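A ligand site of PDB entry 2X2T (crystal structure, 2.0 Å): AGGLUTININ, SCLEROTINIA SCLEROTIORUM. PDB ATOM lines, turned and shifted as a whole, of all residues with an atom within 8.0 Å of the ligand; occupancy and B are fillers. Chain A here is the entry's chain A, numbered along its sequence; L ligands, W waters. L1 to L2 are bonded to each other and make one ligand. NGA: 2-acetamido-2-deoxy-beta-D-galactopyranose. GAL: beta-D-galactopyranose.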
ATOM      1  N   ASN A  20      12.595   4.438 -15.405  1.00  0.00           N
ATOM      2  CA  ASN A  20      11.899   4.897 -16.596  1.00  0.00           C
ATOM      3  C   ASN A  20      12.857   5.391 -17.677  1.00  0.00           C
ATOM      4  O   ASN A  20      14.070   5.415 -17.487  1.00  0.00           O
ATOM      5  CB  ASN A  20      10.842   5.926 -16.225  1.00  0.00           C
ATOM      6  CG  ASN A  20      11.428   7.210 -15.644  1.00  0.00           C
ATOM      7  OD1 ASN A  20      12.596   7.543 -15.871  1.00  0.00           O
ATOM      8  ND2 ASN A  20      10.608   7.953 -14.916  1.00  0.00           N
ATOM      9  N   ASN A  22      14.650   8.091 -19.722  1.00  0.00           N
ATOM     10  CA  ASN A  22      15.207   9.369 -19.219  1.00  0.00           C
ATOM     11  C   ASN A  22      16.137  10.033 -20.256  1.00  0.00           C
ATOM     12  O   ASN A  22      17.085   9.414 -20.693  1.00  0.00           O
ATOM     13  CB  ASN A  22      15.992   9.075 -17.925  1.00  0.00           C
ATOM     14  CG  ASN A  22      16.563  10.330 -17.249  1.00  0.00           C
ATOM     15  OD1 ASN A  22      17.484  10.953 -17.767  1.00  0.00           O
ATOM     16  ND2 ASN A  22      16.024  10.685 -16.079  1.00  0.00           N
ATOM     17  N   ALA A  23      15.844  11.281 -20.631  1.00  0.00           N
ATOM     18  CA  ALA A  23      16.697  12.092 -21.478  1.00  0.00           C
ATOM     19  C   ALA A  23      17.825  12.585 -20.585  1.00  0.00           C
ATOM     20  O   ALA A  23      17.616  13.475 -19.767  1.00  0.00           O
ATOM     21  CB  ALA A  23      15.937  13.291 -22.071  1.00  0.00           C
ATOM     22  N   TRP A  24      18.991  11.993 -20.760  1.00  0.00           N
ATOM     23  CA  TRP A  24      20.122  12.103 -19.821  1.00  0.00           C
ATOM     24  C   TRP A  24      20.588  13.541 -19.668  1.00  0.00           C
ATOM     25  O   TRP A  24      20.827  14.231 -20.659  1.00  0.00           O
ATOM     26  CB  TRP A  24      21.289  11.254 -20.331  1.00  0.00           C
ATOM     27  CG  TRP A  24      22.288  10.800 -19.297  1.00  0.00           C
ATOM     28  CD1 TRP A  24      23.603  11.163 -19.208  1.00  0.00           C
ATOM     29  CD2 TRP A  24      22.059   9.861 -18.247  1.00  0.00           C
ATOM     30  NE1 TRP A  24      24.204  10.504 -18.163  1.00  0.00           N
ATOM     31  CE2 TRP A  24      23.275   9.700 -17.558  1.00  0.00           C
ATOM     32  CE3 TRP A  24      20.942   9.145 -17.828  1.00  0.00           C
ATOM     33  CZ2 TRP A  24      23.402   8.846 -16.453  1.00  0.00           C
ATOM     34  CZ3 TRP A  24      21.070   8.284 -16.735  1.00  0.00           C
ATOM     35  CH2 TRP A  24      22.299   8.141 -16.065  1.00  0.00           C
ATOM     36  N   GLU A  25      20.677  13.984 -18.407  1.00  0.00           N
ATOM     37  CA  GLU A  25      21.069  15.336 -18.000  1.00  0.00           C
ATOM     38  C   GLU A  25      19.898  16.330 -17.953  1.00  0.00           C
ATOM     39  O   GLU A  25      19.992  17.325 -17.267  1.00  0.00           O
ATOM     40  CB  GLU A  25      22.229  15.937 -18.809  1.00  0.00           C
ATOM     41  CG  GLU A  25      23.463  15.063 -18.883  1.00  0.00           C
ATOM     42  CD  GLU A  25      24.694  15.818 -19.379  1.00  0.00           C
ATOM     43  OE1 GLU A  25      25.129  16.783 -18.726  1.00  0.00           O
ATOM     44  OE2 GLU A  25      25.236  15.419 -20.414  1.00  0.00           O
ATOM     45  N   GLY A  26      18.814  16.052 -18.683  1.00  0.00           N
ATOM     46  CA  GLY A  26      17.586  16.849 -18.572  1.00  0.00           C
ATOM     47  C   GLY A  26      17.780  18.308 -18.903  1.00  0.00           C
ATOM     48  O   GLY A  26      17.205  19.202 -18.245  1.00  0.00           O
ATOM     49  N   LYS A  27      18.623  18.563 -19.901  1.00  0.00           N
ATOM     50  CA  LYS A  27      18.932  19.909 -20.385  1.00  0.00           C
ATOM     51  C   LYS A  27      18.073  20.295 -21.582  1.00  0.00           C
ATOM     52  O   LYS A  27      17.411  19.448 -22.180  1.00  0.00           O
ATOM     53  CB  LYS A  27      20.394  19.990 -20.779  1.00  0.00           C
ATOM     54  CG  LYS A  27      21.356  19.881 -19.624  1.00  0.00           C
ATOM     55  CD  LYS A  27      22.742  19.645 -20.152  1.00  0.00           C
ATOM     56  CE  LYS A  27      23.783  19.977 -19.129  1.00  0.00           C
ATOM     57  NZ  LYS A  27      25.141  19.806 -19.731  1.00  0.00           N
ATOM     58  N   VAL A  33      21.321  11.933 -25.161  1.00  0.00           N
ATOM     59  CA  VAL A  33      21.098  10.480 -25.263  1.00  0.00           C
ATOM     60  C   VAL A  33      20.066  10.043 -24.217  1.00  0.00           C
ATOM     61  O   VAL A  33      19.757  10.788 -23.257  1.00  0.00           O
ATOM     62  CB  VAL A  33      22.424   9.642 -25.209  1.00  0.00           C
ATOM     63  CG1 VAL A  33      23.378  10.108 -26.289  1.00  0.00           C
ATOM     64  CG2 VAL A  33      23.120   9.747 -23.848  1.00  0.00           C
ATOM     65  N   ARG A  35      18.610   6.999 -21.551  1.00  0.00           N
ATOM     66  CA  ARG A  35      18.959   5.870 -20.722  1.00  0.00           C
ATOM     67  C   ARG A  35      17.792   5.524 -19.787  1.00  0.00           C
ATOM     68  O   ARG A  35      16.868   6.306 -19.630  1.00  0.00           O
ATOM     69  CB  ARG A  35      20.207   6.153 -19.881  1.00  0.00           C
ATOM     70  CG  ARG A  35      21.444   6.451 -20.711  1.00  0.00           C
ATOM     71  CD  ARG A  35      22.758   6.316 -19.946  1.00  0.00           C
ATOM     72  NE  ARG A  35      23.883   6.303 -20.877  1.00  0.00           N
ATOM     73  CZ  ARG A  35      24.588   7.365 -21.282  1.00  0.00           C
ATOM     74  NH1 ARG A  35      25.566   7.202 -22.154  1.00  0.00           N
ATOM     75  NH2 ARG A  35      24.325   8.582 -20.834  1.00  0.00           N
ATOM     76  N   THR A  36      17.856   4.359 -19.154  1.00  0.00           N
ATOM     77  CA  THR A  36      17.023   4.102 -18.006  1.00  0.00           C
ATOM     78  C   THR A  36      17.577   4.875 -16.796  1.00  0.00           C
ATOM     79  O   THR A  36      18.805   5.123 -16.678  1.00  0.00           O
ATOM     80  CB  THR A  36      16.922   2.580 -17.694  1.00  0.00           C
ATOM     81  OG1 THR A  36      18.175   2.113 -17.196  1.00  0.00           O
ATOM     82  CG2 THR A  36      16.504   1.766 -18.939  1.00  0.00           C
ATOM     83  N   TYR A  37      16.672   5.280 -15.887  1.00  0.00           N
ATOM     84  CA  TYR A  37      17.061   5.976 -14.653  1.00  0.00           C
ATOM     85  C   TYR A  37      15.995   5.764 -13.628  1.00  0.00           C
ATOM     86  O   TYR A  37      14.802   5.595 -13.967  1.00  0.00           O
ATOM     87  CB  TYR A  37      17.218   7.471 -14.912  1.00  0.00           C
ATOM     88  CG  TYR A  37      17.998   8.279 -13.894  1.00  0.00           C
ATOM     89  CD1 TYR A  37      19.370   8.082 -13.725  1.00  0.00           C
ATOM     90  CD2 TYR A  37      17.382   9.297 -13.138  1.00  0.00           C
ATOM     91  CE1 TYR A  37      20.118   8.873 -12.849  1.00  0.00           C
ATOM     92  CE2 TYR A  37      18.147  10.108 -12.247  1.00  0.00           C
ATOM     93  CZ  TYR A  37      19.514   9.874 -12.122  1.00  0.00           C
ATOM     94  OH  TYR A  37      20.314  10.608 -11.267  1.00  0.00           O
ATOM     95  N   THR A  38      16.406   5.823 -12.371  1.00  0.00           N
ATOM     96  CA  THR A  38      15.483   5.776 -11.243  1.00  0.00           C
ATOM     97  C   THR A  38      14.256   6.688 -11.443  1.00  0.00           C
ATOM     98  O   THR A  38      14.392   7.884 -11.760  1.00  0.00           O
ATOM     99  CB  THR A  38      16.209   6.195  -9.953  1.00  0.00           C
ATOM    100  OG1 THR A  38      17.361   5.363  -9.777  1.00  0.00           O
ATOM    101  CG2 THR A  38      15.273   6.075  -8.734  1.00  0.00           C
ATOM    102  N   ARG A  39      13.046   6.130 -11.252  1.00  0.00           N
ATOM    103  CA  ARG A  39      11.803   6.933 -11.389  1.00  0.00           C
ATOM    104  C   ARG A  39      11.698   8.062 -10.344  1.00  0.00           C
ATOM    105  O   ARG A  39      11.408   9.197 -10.692  1.00  0.00           O
ATOM    106  CB  ARG A  39      10.527   6.057 -11.321  1.00  0.00           C
ATOM    107  CG  ARG A  39      10.414   5.135 -12.518  1.00  0.00           C
ATOM    108  CD  ARG A  39       9.268   4.110 -12.395  1.00  0.00           C
ATOM    109  NE  ARG A  39       7.967   4.713 -12.683  1.00  0.00           N
ATOM    110  CZ  ARG A  39       6.835   4.032 -12.809  1.00  0.00           C
ATOM    111  NH1 ARG A  39       6.807   2.715 -12.667  1.00  0.00           N
ATOM    112  NH2 ARG A  39       5.705   4.693 -13.081  1.00  0.00           N
ATOM    113  N   SER A  44      10.570  13.275 -13.089  1.00  0.00           N
ATOM    114  CA  SER A  44      10.960  14.596 -13.551  1.00  0.00           C
ATOM    115  C   SER A  44      10.530  14.752 -15.011  1.00  0.00           C
ATOM    116  O   SER A  44      10.342  13.754 -15.710  1.00  0.00           O
ATOM    117  CB  SER A  44      12.459  14.739 -13.393  1.00  0.00           C
ATOM    118  OG  SER A  44      13.106  13.712 -14.112  1.00  0.00           O
ATOM    119  N   ASP A  45      10.406  15.997 -15.466  1.00  0.00           N
ATOM    120  CA  ASP A  45       9.916  16.265 -16.829  1.00  0.00           C
ATOM    121  C   ASP A  45      10.801  15.703 -17.946  1.00  0.00           C
ATOM    122  O   ASP A  45      10.318  15.369 -19.020  1.00  0.00           O
ATOM    123  CB  ASP A  45       9.710  17.773 -17.046  1.00  0.00           C
ATOM    124  CG  ASP A  45       8.429  18.308 -16.393  1.00  0.00           C
ATOM    125  OD1 ASP A  45       7.638  17.513 -15.831  1.00  0.00           O
ATOM    126  OD2 ASP A  45       8.217  19.524 -16.438  1.00  0.00           O
ATOM    127  N   ASN A  46      12.095  15.605 -17.702  1.00  0.00           N
ATOM    128  CA  ASN A  46      12.981  14.986 -18.684  1.00  0.00           C
ATOM    129  C   ASN A  46      12.766  13.461 -18.779  1.00  0.00           C
ATOM    130  O   ASN A  46      13.338  12.829 -19.659  1.00  0.00           O
ATOM    131  CB  ASN A  46      14.476  15.299 -18.409  1.00  0.00           C
ATOM    132  CG  ASN A  46      14.988  14.683 -17.106  1.00  0.00           C
ATOM    133  OD1 ASN A  46      14.399  14.890 -16.043  1.00  0.00           O
ATOM    134  ND2 ASN A  46      16.119  13.942 -17.186  1.00  0.00           N
ATOM    135  N   ALA A  47      11.956  12.897 -17.867  1.00  0.00           N
ATOM    136  CA  ALA A  47      11.622  11.468 -17.918  1.00  0.00           C
ATOM    137  C   ALA A  47      10.107  11.248 -18.095  1.00  0.00           C
ATOM    138  O   ALA A  47       9.567  10.214 -17.690  1.00  0.00           O
ATOM    139  CB  ALA A  47      12.161  10.740 -16.655  1.00  0.00           C
ATOM    140  N   SER A 131      19.528   1.250 -12.842  1.00  0.00           N
ATOM    141  CA  SER A 131      19.551   2.631 -13.339  1.00  0.00           C
ATOM    142  C   SER A 131      20.829   2.911 -14.150  1.00  0.00           C
ATOM    143  O   SER A 131      21.903   2.394 -13.848  1.00  0.00           O
ATOM    144  CB  SER A 131      19.455   3.630 -12.152  1.00  0.00           C
ATOM    145  OG  SER A 131      19.305   4.978 -12.596  1.00  0.00           O
ATOM    146  N   GLY A 132      20.665   3.743 -15.186  1.00  0.00           N
ATOM    147  CA  GLY A 132      21.794   4.243 -15.965  1.00  0.00           C
ATOM    148  C   GLY A 132      22.216   3.451 -17.186  1.00  0.00           C
ATOM    149  O   GLY A 132      23.298   3.689 -17.708  1.00  0.00           O
HETATM  150  C1  NGA L   1      22.841  18.733 -12.581  1.00  0.00           C
HETATM  151  C2  NGA L   1      21.562  18.008 -13.005  1.00  0.00           C
HETATM  152  C3  NGA L   1      21.860  16.730 -13.786  1.00  0.00           C
HETATM  153  C4  NGA L   1      22.845  17.028 -14.875  1.00  0.00           C
HETATM  154  C5  NGA L   1      24.085  17.708 -14.272  1.00  0.00           C
HETATM  155  C6  NGA L   1      25.109  18.009 -15.348  1.00  0.00           C
HETATM  156  C7  NGA L   1      19.521  18.091 -11.681  1.00  0.00           C
HETATM  157  C8  NGA L   1      18.816  17.664 -10.430  1.00  0.00           C
HETATM  158  N2  NGA L   1      20.750  17.662 -11.862  1.00  0.00           N
HETATM  159  O1  NGA L   1      22.513  19.965 -11.964  1.00  0.00           O
HETATM  160  O3  NGA L   1      20.633  16.244 -14.303  1.00  0.00           O
HETATM  161  O4  NGA L   1      22.232  17.929 -15.810  1.00  0.00           O
HETATM  162  O5  NGA L   1      23.654  18.951 -13.715  1.00  0.00           O
HETATM  163  O6  NGA L   1      25.635  16.783 -15.892  1.00  0.00           O
HETATM  164  O7  NGA L   1      18.996  18.815 -12.498  1.00  0.00           O
HETATM  165  C1  GAL L   2      20.377  14.861 -14.026  1.00  0.00           C
HETATM  166  C2  GAL L   2      18.910  14.560 -14.287  1.00  0.00           C
HETATM  167  C3  GAL L   2      18.623  13.052 -14.207  1.00  0.00           C
HETATM  168  C4  GAL L   2      19.639  12.272 -15.040  1.00  0.00           C
HETATM  169  C5  GAL L   2      21.049  12.680 -14.620  1.00  0.00           C
HETATM  170  C6  GAL L   2      22.122  11.883 -15.354  1.00  0.00           C
HETATM  171  O2  GAL L   2      18.061  15.293 -13.377  1.00  0.00           O
HETATM  172  O3  GAL L   2      17.272  12.800 -14.620  1.00  0.00           O
HETATM  173  O4  GAL L   2      19.425  12.495 -16.448  1.00  0.00           O
HETATM  174  O5  GAL L   2      21.217  14.088 -14.895  1.00  0.00           O
HETATM  175  O6  GAL L   2      23.426  12.140 -14.797  1.00  0.00           O
HETATM  176  O   HOH W   1      24.963  14.259 -15.875  1.00  0.00           O
HETATM  177  O   HOH W   2      25.013  20.723 -11.113  1.00  0.00           O
HETATM  178  O   HOH W   3      22.879  19.732  -9.324  1.00  0.00           O
HETATM  179  O   HOH W   4      15.850  16.585 -14.470  1.00  0.00           O
HETATM  180  O   HOH W   5      27.447  17.926 -18.600  1.00  0.00           O
HETATM  181  O   HOH W   6      22.035  20.732 -16.079  1.00  0.00           O
HETATM  182  O   HOH W   7      15.560  12.719 -12.489  1.00  0.00           O
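ND2 of Asn 46 sits at hydrogen-bond distance from O3 of GAL L2 (3.0 Å). OD1 of Asn 22 sits at hydrogen-bond distance from O4 of GAL L2. N of Glu 25 sits at hydrogen-bond distance from O4 of GAL L2, 2.8 Å away. O of Glu 25 is in hydrogen-bond range of O4 of NGA L1, at 2.7 Å. OE1 of Glu 25 sits at hydrogen-bond distance from O6 of NGA L1, 2.9 Å away.
Water W7 bridges O3 of GAL L2 (2.7 Å) and OG of Ser 44 (3.1 Å). Water W4 lies within hydrogen-bond range of OD1 of Asn 46 (2.7 Å) and O2 of GAL L2 (2.8 Å). Water W5 lies within hydrogen-bond range of the side-chain carboxylate (OE1) of Glu 25 (2.6 Å), the side-chain amino group (NZ) of Lys 27 (3.2 Å) and an oxygen (O6) of NGA L1 (3.5 Å).
Merely in contact with the ligand: Ala 23 (3.9 Å), Trp 24 (3.3 Å) and Tyr 37 (3.6 Å). Hydrophobic or aromatic side chains that line the ligand: Trp 24 and Tyr 37. The nearest printed residue that does not touch the ligand is Lys 27 (4.2 Å).
N of Trp 24 sits at hydrogen-bond distance from O of Val 33 (2.9 Å). The backbone NH of Asn 20 lies within hydrogen-bond range of the backbone carbonyl oxygen of Tyr 37 (2.9 Å). The side-chain hydroxyl of Ser 44 sits at hydrogen-bond distance from the side-chain amide oxygen of Asn 46 (2.6 Å). The backbone carbonyl oxygen (O) of Arg 35 sits at hydrogen-bond distance from the backbone NH (N) of Asn 22, at 2.8 Å. The side-chain amide oxygen (OD1) of Asn 22 sits at hydrogen-bond distance from the side-chain amide nitrogen (ND2) of Asn 46 (3.3 Å). The side-chain amide nitrogen of Asn 46 lies within hydrogen-bond range of the backbone carbonyl oxygen of Ala 23 (3.0 Å). OE1 of Glu 25 lies within salt-bridge range of NZ of Lys 27 (3.2 Å).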
